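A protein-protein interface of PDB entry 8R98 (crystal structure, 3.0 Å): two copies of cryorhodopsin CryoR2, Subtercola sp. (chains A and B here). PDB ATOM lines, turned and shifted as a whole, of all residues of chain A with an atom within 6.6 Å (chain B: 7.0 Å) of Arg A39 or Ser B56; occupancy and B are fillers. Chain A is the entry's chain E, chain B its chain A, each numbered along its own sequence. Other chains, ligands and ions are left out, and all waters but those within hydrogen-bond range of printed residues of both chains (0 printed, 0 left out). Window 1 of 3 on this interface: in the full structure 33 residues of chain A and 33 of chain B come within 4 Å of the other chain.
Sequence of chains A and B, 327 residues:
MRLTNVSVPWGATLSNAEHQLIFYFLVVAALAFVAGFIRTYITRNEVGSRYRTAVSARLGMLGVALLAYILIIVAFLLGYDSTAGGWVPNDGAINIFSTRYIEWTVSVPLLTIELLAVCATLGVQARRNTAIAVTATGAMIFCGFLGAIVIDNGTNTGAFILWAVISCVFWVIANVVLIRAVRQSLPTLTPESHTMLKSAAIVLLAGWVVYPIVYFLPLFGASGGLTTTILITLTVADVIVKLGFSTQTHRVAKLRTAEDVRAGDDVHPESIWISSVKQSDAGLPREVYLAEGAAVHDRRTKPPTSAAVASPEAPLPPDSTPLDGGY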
ATOM      1  N   PHE A  33     -29.569  -1.501  29.227  1.00  0.00           N
ATOM      2  CA  PHE A  33     -28.154  -1.208  28.868  1.00  0.00           C
ATOM      3  C   PHE A  33     -27.661  -2.256  27.865  1.00  0.00           C
ATOM      4  O   PHE A  33     -26.984  -1.875  26.886  1.00  0.00           O
ATOM      5  CB  PHE A  33     -27.269  -1.143  30.116  1.00  0.00           C
ATOM      6  CG  PHE A  33     -27.545   0.039  31.009  1.00  0.00           C
ATOM      7  CD1 PHE A  33     -27.466   1.330  30.512  1.00  0.00           C
ATOM      8  CD2 PHE A  33     -27.870  -0.132  32.345  1.00  0.00           C
ATOM      9  CE1 PHE A  33     -27.723   2.424  31.324  1.00  0.00           C
ATOM     10  CE2 PHE A  33     -28.129   0.961  33.157  1.00  0.00           C
ATOM     11  CZ  PHE A  33     -28.051   2.236  32.647  1.00  0.00           C
ATOM     12  N   VAL A  34     -27.993  -3.529  28.100  1.00  0.00           N
ATOM     13  CA  VAL A  34     -27.632  -4.665  27.200  1.00  0.00           C
ATOM     14  C   VAL A  34     -28.173  -4.348  25.803  1.00  0.00           C
ATOM     15  O   VAL A  34     -27.397  -4.443  24.829  1.00  0.00           O
ATOM     16  CB  VAL A  34     -28.180  -6.007  27.719  1.00  0.00           C
ATOM     17  CG1 VAL A  34     -27.927  -7.133  26.730  1.00  0.00           C
ATOM     18  CG2 VAL A  34     -27.621  -6.355  29.091  1.00  0.00           C
ATOM     19  N   ALA A  35     -29.456  -3.979  25.728  1.00  0.00           N
ATOM     20  CA  ALA A  35     -30.169  -3.592  24.489  1.00  0.00           C
ATOM     21  C   ALA A  35     -29.451  -2.401  23.848  1.00  0.00           C
ATOM     22  O   ALA A  35     -29.235  -2.429  22.620  1.00  0.00           O
ATOM     23  CB  ALA A  35     -31.607  -3.259  24.802  1.00  0.00           C
ATOM     24  N   GLY A  36     -29.103  -1.401  24.665  1.00  0.00           N
ATOM     25  CA  GLY A  36     -28.379  -0.188  24.242  1.00  0.00           C
ATOM     26  C   GLY A  36     -27.001  -0.535  23.706  1.00  0.00           C
ATOM     27  O   GLY A  36     -26.672  -0.088  22.585  1.00  0.00           O
ATOM     28  N   PHE A  37     -26.235  -1.318  24.472  1.00  0.00           N
ATOM     29  CA  PHE A  37     -24.858  -1.764  24.126  1.00  0.00           C
ATOM     30  C   PHE A  37     -24.882  -2.464  22.762  1.00  0.00           C
ATOM     31  O   PHE A  37     -24.036  -2.140  21.902  1.00  0.00           O
ATOM     32  CB  PHE A  37     -24.289  -2.691  25.203  1.00  0.00           C
ATOM     33  CG  PHE A  37     -22.875  -3.149  24.940  1.00  0.00           C
ATOM     34  CD1 PHE A  37     -21.793  -2.479  25.489  1.00  0.00           C
ATOM     35  CD2 PHE A  37     -22.625  -4.244  24.127  1.00  0.00           C
ATOM     36  CE1 PHE A  37     -20.497  -2.901  25.243  1.00  0.00           C
ATOM     37  CE2 PHE A  37     -21.327  -4.662  23.878  1.00  0.00           C
ATOM     38  CZ  PHE A  37     -20.266  -3.991  24.436  1.00  0.00           C
ATOM     39  N   ILE A  38     -25.823  -3.396  22.583  1.00  0.00           N
ATOM     40  CA  ILE A  38     -26.000  -4.178  21.322  1.00  0.00           C
ATOM     41  C   ILE A  38     -26.255  -3.204  20.169  1.00  0.00           C
ATOM     42  O   ILE A  38     -25.559  -3.310  19.136  1.00  0.00           O
ATOM     43  CB  ILE A  38     -27.140  -5.206  21.461  1.00  0.00           C
ATOM     44  CG1 ILE A  38     -26.820  -6.263  22.521  1.00  0.00           C
ATOM     45  CG2 ILE A  38     -27.459  -5.839  20.113  1.00  0.00           C
ATOM     46  CD1 ILE A  38     -27.903  -7.298  22.706  1.00  0.00           C
ATOM     47  N   ARG A  39     -27.215  -2.292  20.345  1.00  0.00           N
ATOM     48  CA  ARG A  39     -27.589  -1.293  19.308  1.00  0.00           C
ATOM     49  C   ARG A  39     -26.361  -0.460  18.936  1.00  0.00           C
ATOM     50  O   ARG A  39     -26.039  -0.389  17.735  1.00  0.00           O
ATOM     51  CB  ARG A  39     -28.710  -0.374  19.797  1.00  0.00           C
ATOM     52  CG  ARG A  39     -29.216   0.587  18.733  1.00  0.00           C
ATOM     53  CD  ARG A  39     -30.539   1.203  19.150  1.00  0.00           C
ATOM     54  NE  ARG A  39     -31.098   2.107  18.156  1.00  0.00           N
ATOM     55  CZ  ARG A  39     -32.277   2.711  18.270  1.00  0.00           C
ATOM     56  NH1 ARG A  39     -33.028   2.505  19.341  1.00  0.00           N
ATOM     57  NH2 ARG A  39     -32.704   3.516  17.315  1.00  0.00           N
ATOM     58  N   THR A  40     -25.703   0.134  19.936  1.00  0.00           N
ATOM     59  CA  THR A  40     -24.506   1.005  19.766  1.00  0.00           C
ATOM     60  C   THR A  40     -23.449   0.281  18.924  1.00  0.00           C
ATOM     61  O   THR A  40     -22.907   0.911  17.994  1.00  0.00           O
ATOM     62  CB  THR A  40     -23.927   1.425  21.123  1.00  0.00           C
ATOM     63  OG1 THR A  40     -24.891   2.249  21.777  1.00  0.00           O
ATOM     64  CG2 THR A  40     -22.619   2.174  21.005  1.00  0.00           C
ATOM     65  N   TYR A  41     -23.170  -0.987  19.248  1.00  0.00           N
ATOM     66  CA  TYR A  41     -22.147  -1.832  18.576  1.00  0.00           C
ATOM     67  C   TYR A  41     -22.515  -2.012  17.099  1.00  0.00           C
ATOM     68  O   TYR A  41     -21.661  -1.736  16.234  1.00  0.00           O
ATOM     69  CB  TYR A  41     -22.000  -3.183  19.285  1.00  0.00           C
ATOM     70  CG  TYR A  41     -20.948  -4.086  18.692  1.00  0.00           C
ATOM     71  CD1 TYR A  41     -21.286  -5.093  17.802  1.00  0.00           C
ATOM     72  CD2 TYR A  41     -19.609  -3.927  19.007  1.00  0.00           C
ATOM     73  CE1 TYR A  41     -20.324  -5.922  17.248  1.00  0.00           C
ATOM     74  CE2 TYR A  41     -18.635  -4.747  18.463  1.00  0.00           C
ATOM     75  CZ  TYR A  41     -18.993  -5.748  17.579  1.00  0.00           C
ATOM     76  OH  TYR A  41     -18.038  -6.562  17.039  1.00  0.00           O
ATOM     77  N   ILE A  42     -23.746  -2.459  16.824  1.00  0.00           N
ATOM     78  CA  ILE A  42     -24.256  -2.719  15.443  1.00  0.00           C
ATOM     79  C   ILE A  42     -24.237  -1.414  14.638  1.00  0.00           C
ATOM     80  O   ILE A  42     -23.873  -1.467  13.447  1.00  0.00           O
ATOM     81  CB  ILE A  42     -25.660  -3.354  15.475  1.00  0.00           C
ATOM     82  CG1 ILE A  42     -25.600  -4.807  15.955  1.00  0.00           C
ATOM     83  CG2 ILE A  42     -26.338  -3.235  14.118  1.00  0.00           C
ATOM     84  CD1 ILE A  42     -26.835  -5.613  15.631  1.00  0.00           C
ATOM     85  N   THR A  43     -24.618  -0.297  15.264  1.00  0.00           N
ATOM     86  CA  THR A  43     -24.658   1.053  14.631  1.00  0.00           C
ATOM     87  C   THR A  43     -23.377   1.815  14.986  1.00  0.00           C
ATOM     88  O   THR A  43     -23.488   2.966  15.468  1.00  0.00           O
ATOM     89  CB  THR A  43     -25.897   1.844  15.072  1.00  0.00           C
ATOM     90  OG1 THR A  43     -25.736   2.187  16.449  1.00  0.00           O
ATOM     91  CG2 THR A  43     -27.187   1.079  14.871  1.00  0.00           C
ATOM     92  N   ARG A  44     -22.212   1.198  14.756  1.00  0.00           N
ATOM     93  CA  ARG A  44     -20.888   1.806  15.062  1.00  0.00           C
ATOM     94  C   ARG A  44     -20.261   2.341  13.770  1.00  0.00           C
ATOM     95  O   ARG A  44     -19.551   3.359  13.841  1.00  0.00           O
ATOM     96  CB  ARG A  44     -19.964   0.789  15.742  1.00  0.00           C
ATOM     97  CG  ARG A  44     -19.456  -0.319  14.830  1.00  0.00           C
ATOM     98  CD  ARG A  44     -18.563  -1.297  15.573  1.00  0.00           C
ATOM     99  NE  ARG A  44     -17.954  -2.293  14.700  1.00  0.00           N
ATOM    100  CZ  ARG A  44     -18.492  -3.472  14.403  1.00  0.00           C
ATOM    101  NH1 ARG A  44     -19.669  -3.812  14.901  1.00  0.00           N
ATOM    102  NH2 ARG A  44     -17.853  -4.306  13.601  1.00  0.00           N
ATOM    103  N   LEU A  59     -20.168   3.252  23.851  1.00  0.00           N
ATOM    104  CA  LEU A  59     -20.139   1.767  23.968  1.00  0.00           C
ATOM    105  C   LEU A  59     -19.464   1.395  25.293  1.00  0.00           C
ATOM    106  O   LEU A  59     -19.980   0.494  25.988  1.00  0.00           O
ATOM    107  CB  LEU A  59     -19.404   1.147  22.775  1.00  0.00           C
ATOM    108  CG  LEU A  59     -19.599  -0.361  22.610  1.00  0.00           C
ATOM    109  CD1 LEU A  59     -21.074  -0.707  22.456  1.00  0.00           C
ATOM    110  CD2 LEU A  59     -18.804  -0.888  21.427  1.00  0.00           C
ATOM    111  N   THR A 247     -28.086   8.691  22.471  1.00  0.00           N
ATOM    112  CA  THR A 247     -28.499   8.871  21.053  1.00  0.00           C
ATOM    113  C   THR A 247     -28.155  10.286  20.592  1.00  0.00           C
ATOM    114  O   THR A 247     -27.620  10.412  19.477  1.00  0.00           O
ATOM    115  CB  THR A 247     -29.996   8.624  20.833  1.00  0.00           C
ATOM    116  OG1 THR A 247     -30.332   7.355  21.394  1.00  0.00           O
ATOM    117  CG2 THR A 247     -30.374   8.664  19.366  1.00  0.00           C
ATOM    118  N   THR B  40     -29.516 -13.963  14.038  1.00  0.00           N
ATOM    119  CA  THR B  40     -29.819 -12.517  13.850  1.00  0.00           C
ATOM    120  C   THR B  40     -28.521 -11.745  13.590  1.00  0.00           C
ATOM    121  O   THR B  40     -28.499 -10.928  12.649  1.00  0.00           O
ATOM    122  CB  THR B  40     -30.558 -11.945  15.067  1.00  0.00           C
ATOM    123  OG1 THR B  40     -31.834 -12.581  15.146  1.00  0.00           O
ATOM    124  CG2 THR B  40     -30.743 -10.444  15.002  1.00  0.00           C
ATOM    125  N   TYR B  51     -33.067   0.566   7.374  1.00  0.00           N
ATOM    126  CA  TYR B  51     -33.914  -0.341   8.195  1.00  0.00           C
ATOM    127  C   TYR B  51     -33.062  -1.093   9.227  1.00  0.00           C
ATOM    128  O   TYR B  51     -33.537  -2.126   9.746  1.00  0.00           O
ATOM    129  CB  TYR B  51     -34.660  -1.323   7.285  1.00  0.00           C
ATOM    130  CG  TYR B  51     -35.250  -0.695   6.045  1.00  0.00           C
ATOM    131  CD1 TYR B  51     -36.435   0.023   6.095  1.00  0.00           C
ATOM    132  CD2 TYR B  51     -34.617  -0.814   4.818  1.00  0.00           C
ATOM    133  CE1 TYR B  51     -36.975   0.608   4.959  1.00  0.00           C
ATOM    134  CE2 TYR B  51     -35.140  -0.231   3.673  1.00  0.00           C
ATOM    135  CZ  TYR B  51     -36.320   0.483   3.746  1.00  0.00           C
ATOM    136  OH  TYR B  51     -36.824   1.059   2.618  1.00  0.00           O
ATOM    137  N   ARG B  52     -31.859  -0.595   9.528  1.00  0.00           N
ATOM    138  CA  ARG B  52     -30.915  -1.268  10.465  1.00  0.00           C
ATOM    139  C   ARG B  52     -31.501  -1.269  11.880  1.00  0.00           C
ATOM    140  O   ARG B  52     -31.174  -2.202  12.649  1.00  0.00           O
ATOM    141  CB  ARG B  52     -29.534  -0.607  10.472  1.00  0.00           C
ATOM    142  CG  ARG B  52     -28.507  -1.377  11.294  1.00  0.00           C
ATOM    143  CD  ARG B  52     -27.098  -0.871  11.092  1.00  0.00           C
ATOM    144  NE  ARG B  52     -26.726  -0.948   9.688  1.00  0.00           N
ATOM    145  CZ  ARG B  52     -25.642  -0.392   9.163  1.00  0.00           C
ATOM    146  NH1 ARG B  52     -24.808   0.292   9.929  1.00  0.00           N
ATOM    147  NH2 ARG B  52     -25.404  -0.514   7.869  1.00  0.00           N
ATOM    148  N   THR B  53     -32.321  -0.268  12.214  1.00  0.00           N
ATOM    149  CA  THR B  53     -32.949  -0.141  13.557  1.00  0.00           C
ATOM    150  C   THR B  53     -33.717  -1.428  13.871  1.00  0.00           C
ATOM    151  O   THR B  53     -33.717  -1.834  15.047  1.00  0.00           O
ATOM    152  CB  THR B  53     -33.869   1.080  13.668  1.00  0.00           C
ATOM    153  OG1 THR B  53     -33.147   2.224  13.214  1.00  0.00           O
ATOM    154  CG2 THR B  53     -34.362   1.305  15.082  1.00  0.00           C
ATOM    155  N   ALA B  54     -34.342  -2.032  12.854  1.00  0.00           N
ATOM    156  CA  ALA B  54     -35.108  -3.295  12.961  1.00  0.00           C
ATOM    157  C   ALA B  54     -34.184  -4.411  13.465  1.00  0.00           C
ATOM    158  O   ALA B  54     -34.573  -5.124  14.406  1.00  0.00           O
ATOM    159  CB  ALA B  54     -35.721  -3.640  11.626  1.00  0.00           C
ATOM    160  N   VAL B  55     -32.996  -4.541  12.866  1.00  0.00           N
ATOM    161  CA  VAL B  55     -31.978  -5.575  13.227  1.00  0.00           C
ATOM    162  C   VAL B  55     -31.507  -5.326  14.666  1.00  0.00           C
ATOM    163  O   VAL B  55     -31.538  -6.274  15.480  1.00  0.00           O
ATOM    164  CB  VAL B  55     -30.793  -5.575  12.242  1.00  0.00           C
ATOM    165  CG1 VAL B  55     -29.753  -6.618  12.621  1.00  0.00           C
ATOM    166  CG2 VAL B  55     -31.250  -5.779  10.805  1.00  0.00           C
ATOM    167  N   SER B  56     -31.082  -4.094  14.963  1.00  0.00           N
ATOM    168  CA  SER B  56     -30.590  -3.667  16.301  1.00  0.00           C
ATOM    169  C   SER B  56     -31.615  -4.018  17.388  1.00  0.00           C
ATOM    170  O   SER B  56     -31.204  -4.557  18.436  1.00  0.00           O
ATOM    171  CB  SER B  56     -30.268  -2.199  16.323  1.00  0.00           C
ATOM    172  OG  SER B  56     -31.414  -1.422  16.013  1.00  0.00           O
ATOM    173  N   ALA B  57     -32.893  -3.716  17.144  1.00  0.00           N
ATOM    174  CA  ALA B  57     -34.020  -3.940  18.082  1.00  0.00           C
ATOM    175  C   ALA B  57     -34.171  -5.438  18.364  1.00  0.00           C
ATOM    176  O   ALA B  57     -34.190  -5.810  19.552  1.00  0.00           O
ATOM    177  CB  ALA B  57     -35.295  -3.362  17.518  1.00  0.00           C
ATOM    178  N   ARG B  58     -34.268  -6.261  17.316  1.00  0.00           N
ATOM    179  CA  ARG B  58     -34.483  -7.725  17.457  1.00  0.00           C
ATOM    180  C   ARG B  58     -33.305  -8.341  18.220  1.00  0.00           C
ATOM    181  O   ARG B  58     -33.561  -9.060  19.207  1.00  0.00           O
ATOM    182  CB  ARG B  58     -34.690  -8.385  16.091  1.00  0.00           C
ATOM    183  CG  ARG B  58     -35.188  -9.820  16.175  1.00  0.00           C
ATOM    184  CD  ARG B  58     -36.396  -9.980  17.087  1.00  0.00           C
ATOM    185  NE  ARG B  58     -37.638  -9.483  16.510  1.00  0.00           N
ATOM    186  CZ  ARG B  58     -38.849  -9.755  16.985  1.00  0.00           C
ATOM    187  NH1 ARG B  58     -39.917  -9.261  16.384  1.00  0.00           N
ATOM    188  NH2 ARG B  58     -38.987 -10.531  18.046  1.00  0.00           N
ATOM    189  N   LEU B  59     -32.069  -8.067  17.791  1.00  0.00           N
ATOM    190  CA  LEU B  59     -30.851  -8.610  18.449  1.00  0.00           C
ATOM    191  C   LEU B  59     -30.895  -8.236  19.937  1.00  0.00           C
ATOM    192  O   LEU B  59     -30.586  -9.105  20.775  1.00  0.00           O
ATOM    193  CB  LEU B  59     -29.595  -8.063  17.767  1.00  0.00           C
ATOM    194  CG  LEU B  59     -28.307  -8.807  18.119  1.00  0.00           C
ATOM    195  CD1 LEU B  59     -28.416 -10.273  17.738  1.00  0.00           C
ATOM    196  CD2 LEU B  59     -27.097  -8.173  17.453  1.00  0.00           C
ATOM    197  N   GLY B  60     -31.278  -6.993  20.242  1.00  0.00           N
ATOM    198  CA  GLY B  60     -31.434  -6.490  21.621  1.00  0.00           C
ATOM    199  C   GLY B  60     -32.467  -7.300  22.386  1.00  0.00           C
ATOM    200  O   GLY B  60     -32.144  -7.788  23.484  1.00  0.00           O
ATOM    201  N   MET B  61     -33.665  -7.446  21.815  1.00  0.00           N
ATOM    202  CA  MET B  61     -34.796  -8.220  22.395  1.00  0.00           C
ATOM    203  C   MET B  61     -34.315  -9.632  22.749  1.00  0.00           C
ATOM    204  O   MET B  61     -34.516 -10.060  23.905  1.00  0.00           O
ATOM    205  CB  MET B  61     -35.954  -8.315  21.398  1.00  0.00           C
ATOM    206  CG  MET B  61     -37.108  -9.170  21.880  1.00  0.00           C
ATOM    207  SD  MET B  61     -38.371  -9.404  20.602  1.00  0.00           S
ATOM    208  CE  MET B  61     -38.585  -7.721  20.021  1.00  0.00           C
ATOM    209  N   LEU B 110     -39.021  -2.781  22.700  1.00  0.00           N
ATOM    210  CA  LEU B 110     -38.069  -3.017  21.579  1.00  0.00           C
ATOM    211  C   LEU B 110     -38.838  -3.524  20.353  1.00  0.00           C
ATOM    212  O   LEU B 110     -38.553  -3.049  19.236  1.00  0.00           O
ATOM    213  CB  LEU B 110     -37.004  -4.022  22.030  1.00  0.00           C
ATOM    214  CG  LEU B 110     -36.086  -3.530  23.145  1.00  0.00           C
ATOM    215  CD1 LEU B 110     -35.136  -4.630  23.596  1.00  0.00           C
ATOM    216  CD2 LEU B 110     -35.308  -2.308  22.683  1.00  0.00           C
ATOM    217  N   ILE B 113     -40.505  -0.677  18.425  1.00  0.00           N
ATOM    218  CA  ILE B 113     -39.466   0.039  17.626  1.00  0.00           C
ATOM    219  C   ILE B 113     -39.198  -0.752  16.342  1.00  0.00           C
ATOM    220  O   ILE B 113     -39.121  -0.124  15.265  1.00  0.00           O
ATOM    221  CB  ILE B 113     -38.173   0.232  18.445  1.00  0.00           C
ATOM    222  CG1 ILE B 113     -38.462   0.732  19.863  1.00  0.00           C
ATOM    223  CG2 ILE B 113     -37.203   1.144  17.712  1.00  0.00           C
ATOM    224  CD1 ILE B 113     -37.221   0.957  20.699  1.00  0.00           C
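Of chain B, only Thr B53 (3.6 Å) and Ser B56 (3.8 Å) come within 4 Å of Arg A39.
Of chain A, only Arg A39 comes within 4 Å of Ser B56.
Of the printed residues of chain A, Leu B59 touches Ile A38 and Ile A42.
Of the printed residues of chain A, Arg B52 touches Ile A42.
Printed residues of chain B within 4 Å of Ala A35: Leu B110 (3.97 Å).
Printed residues of chain B within 4 Å of Ile A38: Leu B59 (3.6 Å) and Gly B60 (3.8 Å).
The nearest printed residue of chain A that does not touch Ser B56 is Ile A42 (4.3 Å).
The nearest printed residue of chain A that does not touch Gly B60 is Ala A35 (4.3 Å).
Printed residues of chain B that touch a printed residue of chain A: Arg B52, Thr B53, Ser B56, Leu B59, Gly B60 and Leu B110.
Printed residues of chain A that touch a printed residue of chain B: Ala A35, Ile A38, Arg A39 and Ile A42.
Hydrophobic or aromatic side chains of chain A within 4 Å of the printed part of chain B: Ala A35, Ile A38 and Ile A42.
The backbone carbonyl oxygen (O) of Arg B52 sits at hydrogen-bond distance from the side-chain hydroxyl (OG) of Ser B56 (3.5 Å).
The side-chain hydroxyl of Ser B56 is in hydrogen-bond range of the backbone carbonyl oxygen of Thr B53, at 2.5 Å.
The backbone carbonyl oxygen (O) of Arg A39 sits at hydrogen-bond distance from the side-chain hydroxyl (OG1) of Thr A43, 2.9 Å away.
Among the printed residues, merely in contact across the chains: Ala A35 with Leu B110 (3.97 Å), Ile A38 with Leu B59 (3.6 Å), Ile A38 with Gly B60 (3.8 Å), Arg A39 with Thr B53 (3.6 Å), Arg A39 with Ser B56 (3.8 Å), Ile A42 with Arg B52 (3.9 Å) and Ile A42 with Leu B59 (3.2 Å).
Positions printed for both chains: 40 and 59.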
